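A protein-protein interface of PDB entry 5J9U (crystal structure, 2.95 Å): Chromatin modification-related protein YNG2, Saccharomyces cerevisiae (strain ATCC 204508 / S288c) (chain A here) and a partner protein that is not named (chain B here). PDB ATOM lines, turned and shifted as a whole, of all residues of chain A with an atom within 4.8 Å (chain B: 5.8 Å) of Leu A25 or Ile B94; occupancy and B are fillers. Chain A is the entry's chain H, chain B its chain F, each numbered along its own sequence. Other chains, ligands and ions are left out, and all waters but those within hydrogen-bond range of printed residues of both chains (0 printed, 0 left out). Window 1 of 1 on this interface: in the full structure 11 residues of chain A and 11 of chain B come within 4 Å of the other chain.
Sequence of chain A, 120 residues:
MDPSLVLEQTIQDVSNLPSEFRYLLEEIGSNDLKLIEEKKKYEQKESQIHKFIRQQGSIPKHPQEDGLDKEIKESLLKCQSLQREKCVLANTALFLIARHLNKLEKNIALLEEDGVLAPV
The guanidinium group (NH1) of Arg A22 sits at hydrogen-bond distance from the backbone carbonyl oxygen (O) of Ile B70 (3.0 Å).
The backbone NH of Gly A29 sits close to the backbone carbonyl oxygen of Ser B98 (3.5 Å).
OE2 of Glu B40 sits at hydrogen-bond distance from N of Phe B95, at 3.2 Å.
Among the printed residues, pairs that only touch across the chains: Phe A21 with Ile B69 (3.4 Å), Arg A22 with Ile B69 (3.6 Å), Leu A25 with Ile B94 (3.5 Å), Leu A25 with Phe B95 (3.8 Å), Leu A25 with Ser B98 (3.6 Å) and Ile A28 with Ser B98 (3.4 Å).
Printed residues of chain B within 4 Å of Phe A21: Ile B69 (3.4 Å).
Leu A25 touches just these residues of chain B: Ile B94 (3.5 Å), Phe B95 (3.8 Å) and Ser B98 (3.6 Å).
Printed residues of chain B within 4 Å of Ile A28: Ser B98.
Ile B94 touches one residue of chain A.
Printed residues of chain A within 4 Å of Ser B98: Leu A25 (3.6 Å), Ile A28 (3.4 Å) and Gly A29 (3.4 Å).
The nearest residue of chain A that does not touch Ile B94 is Arg A22 (4.1 Å).
The nearest printed residue of chain B that does not touch Phe A21 is Phe B95 (4.1 Å).
Hydrophobic or aromatic side chains of chain A within 4 Å of the printed part of chain B: Phe A21, Leu A25 and Ile A28.
Hydrophobic or aromatic side chains of chain B within 4 Å of the printed part of chain A: Ile B69, Ile B70, Ile B94 and Phe B95.
Along chain B the printed residues that touch a printed residue of chain A span positions 69 to 98.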
ATOM      1  N   PHE A  21       1.206  22.269   1.600  1.00  0.00           N
ATOM      2  CA  PHE A  21       1.010  20.912   2.096  1.00  0.00           C
ATOM      3  C   PHE A  21      -0.260  20.295   1.528  1.00  0.00           C
ATOM      4  O   PHE A  21      -0.272  19.119   1.149  1.00  0.00           O
ATOM      5  CB  PHE A  21       0.971  20.908   3.624  1.00  0.00           C
ATOM      6  CG  PHE A  21       2.299  20.617   4.258  1.00  0.00           C
ATOM      7  CD1 PHE A  21       2.374  19.997   5.491  1.00  0.00           C
ATOM      8  CD2 PHE A  21       3.475  20.962   3.613  1.00  0.00           C
ATOM      9  CE1 PHE A  21       3.600  19.726   6.071  1.00  0.00           C
ATOM     10  CE2 PHE A  21       4.701  20.698   4.191  1.00  0.00           C
ATOM     11  CZ  PHE A  21       4.763  20.080   5.422  1.00  0.00           C
ATOM     12  N   ARG A  22      -1.342  21.075   1.469  1.00  0.00           N
ATOM     13  CA  ARG A  22      -2.578  20.594   0.862  1.00  0.00           C
ATOM     14  C   ARG A  22      -2.353  20.223  -0.598  1.00  0.00           C
ATOM     15  O   ARG A  22      -2.723  19.130  -1.041  1.00  0.00           O
ATOM     16  CB  ARG A  22      -3.665  21.662   0.989  1.00  0.00           C
ATOM     17  CG  ARG A  22      -4.459  21.575   2.278  1.00  0.00           C
ATOM     18  CD  ARG A  22      -5.698  22.452   2.239  1.00  0.00           C
ATOM     19  NE  ARG A  22      -6.559  22.206   3.391  1.00  0.00           N
ATOM     20  CZ  ARG A  22      -6.339  22.707   4.603  1.00  0.00           C
ATOM     21  NH1 ARG A  22      -5.286  23.484   4.821  1.00  0.00           N
ATOM     22  NH2 ARG A  22      -7.171  22.431   5.598  1.00  0.00           N
ATOM     23  N   TYR A  23      -1.746  21.138  -1.359  1.00  0.00           N
ATOM     24  CA  TYR A  23      -1.476  20.908  -2.775  1.00  0.00           C
ATOM     25  C   TYR A  23      -0.652  19.645  -2.995  1.00  0.00           C
ATOM     26  O   TYR A  23      -0.894  18.895  -3.948  1.00  0.00           O
ATOM     27  CB  TYR A  23      -0.757  22.130  -3.349  1.00  0.00           C
ATOM     28  CG  TYR A  23      -0.340  22.020  -4.797  1.00  0.00           C
ATOM     29  CD1 TYR A  23      -1.217  22.341  -5.822  1.00  0.00           C
ATOM     30  CD2 TYR A  23       0.947  21.620  -5.136  1.00  0.00           C
ATOM     31  CE1 TYR A  23      -0.830  22.252  -7.148  1.00  0.00           C
ATOM     32  CE2 TYR A  23       1.343  21.528  -6.457  1.00  0.00           C
ATOM     33  CZ  TYR A  23       0.451  21.846  -7.457  1.00  0.00           C
ATOM     34  OH  TYR A  23       0.842  21.755  -8.774  1.00  0.00           O
ATOM     35  N   LEU A  24       0.319  19.388  -2.120  1.00  0.00           N
ATOM     36  CA  LEU A  24       1.170  18.211  -2.262  1.00  0.00           C
ATOM     37  C   LEU A  24       0.451  16.937  -1.831  1.00  0.00           C
ATOM     38  O   LEU A  24       0.480  15.929  -2.545  1.00  0.00           O
ATOM     39  CB  LEU A  24       2.453  18.398  -1.451  1.00  0.00           C
ATOM     40  CG  LEU A  24       3.468  19.394  -2.012  1.00  0.00           C
ATOM     41  CD1 LEU A  24       4.664  19.511  -1.083  1.00  0.00           C
ATOM     42  CD2 LEU A  24       3.906  18.977  -3.406  1.00  0.00           C
ATOM     43  N   LEU A  25      -0.187  16.964  -0.658  1.00  0.00           N
ATOM     44  CA  LEU A  25      -0.850  15.769  -0.143  1.00  0.00           C
ATOM     45  C   LEU A  25      -1.994  15.328  -1.049  1.00  0.00           C
ATOM     46  O   LEU A  25      -2.168  14.130  -1.300  1.00  0.00           O
ATOM     47  CB  LEU A  25      -1.348  16.023   1.278  1.00  0.00           C
ATOM     48  CG  LEU A  25      -0.242  16.165   2.327  1.00  0.00           C
ATOM     49  CD1 LEU A  25      -0.826  16.464   3.698  1.00  0.00           C
ATOM     50  CD2 LEU A  25       0.625  14.915   2.366  1.00  0.00           C
ATOM     51  N   GLU A  26      -2.790  16.278  -1.545  1.00  0.00           N
ATOM     52  CA  GLU A  26      -3.888  15.921  -2.436  1.00  0.00           C
ATOM     53  C   GLU A  26      -3.387  15.453  -3.795  1.00  0.00           C
ATOM     54  O   GLU A  26      -4.140  14.808  -4.534  1.00  0.00           O
ATOM     55  CB  GLU A  26      -4.845  17.102  -2.599  1.00  0.00           C
ATOM     56  CG  GLU A  26      -4.398  18.134  -3.618  1.00  0.00           C
ATOM     57  CD  GLU A  26      -5.292  19.356  -3.632  1.00  0.00           C
ATOM     58  OE1 GLU A  26      -6.250  19.398  -2.832  1.00  0.00           O
ATOM     59  OE2 GLU A  26      -5.039  20.271  -4.444  1.00  0.00           O
ATOM     60  N   GLU A  27      -2.135  15.758  -4.136  1.00  0.00           N
ATOM     61  CA  GLU A  27      -1.506  15.170  -5.310  1.00  0.00           C
ATOM     62  C   GLU A  27      -0.988  13.771  -5.017  1.00  0.00           C
ATOM     63  O   GLU A  27      -0.830  12.970  -5.946  1.00  0.00           O
ATOM     64  CB  GLU A  27      -0.369  16.067  -5.805  1.00  0.00           C
ATOM     65  CG  GLU A  27      -0.749  16.997  -6.954  1.00  0.00           C
ATOM     66  CD  GLU A  27      -1.097  16.249  -8.226  1.00  0.00           C
ATOM     67  OE1 GLU A  27      -0.334  15.339  -8.611  1.00  0.00           O
ATOM     68  OE2 GLU A  27      -2.135  16.574  -8.842  1.00  0.00           O
ATOM     69  N   ILE A  28      -0.714  13.469  -3.748  1.00  0.00           N
ATOM     70  CA  ILE A  28      -0.366  12.107  -3.358  1.00  0.00           C
ATOM     71  C   ILE A  28      -1.608  11.228  -3.379  1.00  0.00           C
ATOM     72  O   ILE A  28      -1.599  10.121  -3.930  1.00  0.00           O
ATOM     73  CB  ILE A  28       0.304  12.094  -1.971  1.00  0.00           C
ATOM     74  CG1 ILE A  28       1.691  12.734  -2.034  1.00  0.00           C
ATOM     75  CG2 ILE A  28       0.387  10.671  -1.431  1.00  0.00           C
ATOM     76  CD1 ILE A  28       2.366  12.846  -0.686  1.00  0.00           C
ATOM     77  N   GLY A  29      -2.697  11.711  -2.773  1.00  0.00           N
ATOM     78  CA  GLY A  29      -3.930  10.942  -2.754  1.00  0.00           C
ATOM     79  C   GLY A  29      -4.489  10.689  -4.140  1.00  0.00           C
ATOM     80  O   GLY A  29      -5.064   9.630  -4.402  1.00  0.00           O
ATOM     81  N   GLU B  40      -2.721  13.190  14.160  1.00  0.00           N
ATOM     82  CA  GLU B  40      -3.649  14.230  13.729  1.00  0.00           C
ATOM     83  C   GLU B  40      -4.583  14.621  14.866  1.00  0.00           C
ATOM     84  O   GLU B  40      -4.951  15.792  15.010  1.00  0.00           O
ATOM     85  CB  GLU B  40      -4.467  13.743  12.532  1.00  0.00           C
ATOM     86  CG  GLU B  40      -3.726  13.692  11.210  1.00  0.00           C
ATOM     87  CD  GLU B  40      -4.569  13.066  10.116  1.00  0.00           C
ATOM     88  OE1 GLU B  40      -5.487  12.284  10.447  1.00  0.00           O
ATOM     89  OE2 GLU B  40      -4.317  13.351   8.928  1.00  0.00           O
ATOM     90  N   ILE B  69      -0.916  23.794  10.286  1.00  0.00           N
ATOM     91  CA  ILE B  69      -0.864  23.681   8.835  1.00  0.00           C
ATOM     92  C   ILE B  69      -2.278  23.519   8.298  1.00  0.00           C
ATOM     93  O   ILE B  69      -2.521  23.748   7.104  1.00  0.00           O
ATOM     94  CB  ILE B  69       0.001  22.486   8.395  1.00  0.00           C
ATOM     95  CG1 ILE B  69       1.407  22.588   8.958  1.00  0.00           C
ATOM     96  CG2 ILE B  69       0.119  22.393   6.880  1.00  0.00           C
ATOM     97  CD1 ILE B  69       2.182  21.349   8.684  1.00  0.00           C
ATOM     98  N   ILE B  70      -3.226  23.158   9.161  1.00  0.00           N
ATOM     99  CA  ILE B  70      -4.610  23.017   8.738  1.00  0.00           C
ATOM    100  C   ILE B  70      -5.234  24.388   8.517  1.00  0.00           C
ATOM    101  O   ILE B  70      -5.840  24.653   7.474  1.00  0.00           O
ATOM    102  CB  ILE B  70      -5.399  22.197   9.774  1.00  0.00           C
ATOM    103  CG1 ILE B  70      -4.600  20.964  10.207  1.00  0.00           C
ATOM    104  CG2 ILE B  70      -6.754  21.795   9.214  1.00  0.00           C
ATOM    105  CD1 ILE B  70      -4.253  20.022   9.077  1.00  0.00           C
ATOM    106  N   ASN B  91     -12.791  15.932   7.632  1.00  0.00           N
ATOM    107  CA  ASN B  91     -12.449  16.348   6.281  1.00  0.00           C
ATOM    108  C   ASN B  91     -11.157  17.151   6.237  1.00  0.00           C
ATOM    109  O   ASN B  91     -10.634  17.398   5.146  1.00  0.00           O
ATOM    110  CB  ASN B  91     -13.596  17.177   5.692  1.00  0.00           C
ATOM    111  CG  ASN B  91     -14.949  16.510   5.869  1.00  0.00           C
ATOM    112  OD1 ASN B  91     -15.064  15.284   5.817  1.00  0.00           O
ATOM    113  ND2 ASN B  91     -15.982  17.315   6.099  1.00  0.00           N
ATOM    114  N   ASP B  92     -10.639  17.563   7.394  1.00  0.00           N
ATOM    115  CA  ASP B  92      -9.399  18.318   7.493  1.00  0.00           C
ATOM    116  C   ASP B  92      -8.191  17.447   7.812  1.00  0.00           C
ATOM    117  O   ASP B  92      -7.094  17.981   8.001  1.00  0.00           O
ATOM    118  CB  ASP B  92      -9.534  19.416   8.554  1.00  0.00           C
ATOM    119  CG  ASP B  92     -10.418  20.561   8.098  1.00  0.00           C
ATOM    120  OD1 ASP B  92     -10.597  21.520   8.878  1.00  0.00           O
ATOM    121  OD2 ASP B  92     -10.923  20.508   6.958  1.00  0.00           O
ATOM    122  N   ARG B  93      -8.362  16.125   7.888  1.00  0.00           N
ATOM    123  CA  ARG B  93      -7.255  15.205   8.159  1.00  0.00           C
ATOM    124  C   ARG B  93      -6.462  14.969   6.872  1.00  0.00           C
ATOM    125  O   ARG B  93      -6.415  13.871   6.316  1.00  0.00           O
ATOM    126  CB  ARG B  93      -7.776  13.900   8.745  1.00  0.00           C
ATOM    127  CG  ARG B  93      -8.362  14.027  10.145  1.00  0.00           C
ATOM    128  CD  ARG B  93      -8.836  12.679  10.673  1.00  0.00           C
ATOM    129  NE  ARG B  93      -9.384  12.779  12.024  1.00  0.00           N
ATOM    130  CZ  ARG B  93      -8.705  12.484  13.128  1.00  0.00           C
ATOM    131  NH1 ARG B  93      -7.450  12.065  13.045  1.00  0.00           N
ATOM    132  NH2 ARG B  93      -9.282  12.604  14.316  1.00  0.00           N
ATOM    133  N   ILE B  94      -5.807  16.041   6.412  1.00  0.00           N
ATOM    134  CA  ILE B  94      -5.158  16.045   5.103  1.00  0.00           C
ATOM    135  C   ILE B  94      -4.056  15.001   4.987  1.00  0.00           C
ATOM    136  O   ILE B  94      -3.739  14.561   3.877  1.00  0.00           O
ATOM    137  CB  ILE B  94      -4.601  17.451   4.794  1.00  0.00           C
ATOM    138  CG1 ILE B  94      -3.561  17.855   5.839  1.00  0.00           C
ATOM    139  CG2 ILE B  94      -5.726  18.469   4.742  1.00  0.00           C
ATOM    140  CD1 ILE B  94      -2.781  19.099   5.477  1.00  0.00           C
ATOM    141  N   PHE B  95      -3.461  14.586   6.106  1.00  0.00           N
ATOM    142  CA  PHE B  95      -2.406  13.580   6.040  1.00  0.00           C
ATOM    143  C   PHE B  95      -2.986  12.188   5.835  1.00  0.00           C
ATOM    144  O   PHE B  95      -2.455  11.400   5.045  1.00  0.00           O
ATOM    145  CB  PHE B  95      -1.549  13.628   7.306  1.00  0.00           C
ATOM    146  CG  PHE B  95      -0.864  14.947   7.524  1.00  0.00           C
ATOM    147  CD1 PHE B  95       0.425  15.158   7.066  1.00  0.00           C
ATOM    148  CD2 PHE B  95      -1.511  15.977   8.187  1.00  0.00           C
ATOM    149  CE1 PHE B  95       1.057  16.372   7.266  1.00  0.00           C
ATOM    150  CE2 PHE B  95      -0.887  17.191   8.389  1.00  0.00           C
ATOM    151  CZ  PHE B  95       0.399  17.389   7.930  1.00  0.00           C
ATOM    152  N   SER B  96      -4.072  11.868   6.541  1.00  0.00           N
ATOM    153  CA  SER B  96      -4.726  10.579   6.348  1.00  0.00           C
ATOM    154  C   SER B  96      -5.389  10.507   4.979  1.00  0.00           C
ATOM    155  O   SER B  96      -5.333   9.470   4.308  1.00  0.00           O
ATOM    156  CB  SER B  96      -5.748  10.338   7.458  1.00  0.00           C
ATOM    157  OG  SER B  96      -5.110  10.145   8.708  1.00  0.00           O
ATOM    158  N   LEU B  97      -6.014  11.605   4.546  1.00  0.00           N
ATOM    159  CA  LEU B  97      -6.723  11.642   3.272  1.00  0.00           C
ATOM    160  C   LEU B  97      -5.787  11.597   2.074  1.00  0.00           C
ATOM    161  O   LEU B  97      -6.267  11.623   0.935  1.00  0.00           O
ATOM    162  CB  LEU B  97      -7.598  12.896   3.203  1.00  0.00           C
ATOM    163  CG  LEU B  97      -8.642  13.043   4.313  1.00  0.00           C
ATOM    164  CD1 LEU B  97      -9.161  14.470   4.380  1.00  0.00           C
ATOM    165  CD2 LEU B  97      -9.787  12.063   4.112  1.00  0.00           C
ATOM    166  N   SER B  98      -4.478  11.527   2.299  1.00  0.00           N
ATOM    167  CA  SER B  98      -3.503  11.377   1.230  1.00  0.00           C
ATOM    168  C   SER B  98      -3.240   9.915   0.912  1.00  0.00           C
ATOM    169  O   SER B  98      -2.460   9.616   0.001  1.00  0.00           O
ATOM    170  CB  SER B  98      -2.191  12.075   1.602  1.00  0.00           C
ATOM    171  OG  SER B  98      -1.723  11.642   2.867  1.00  0.00           O
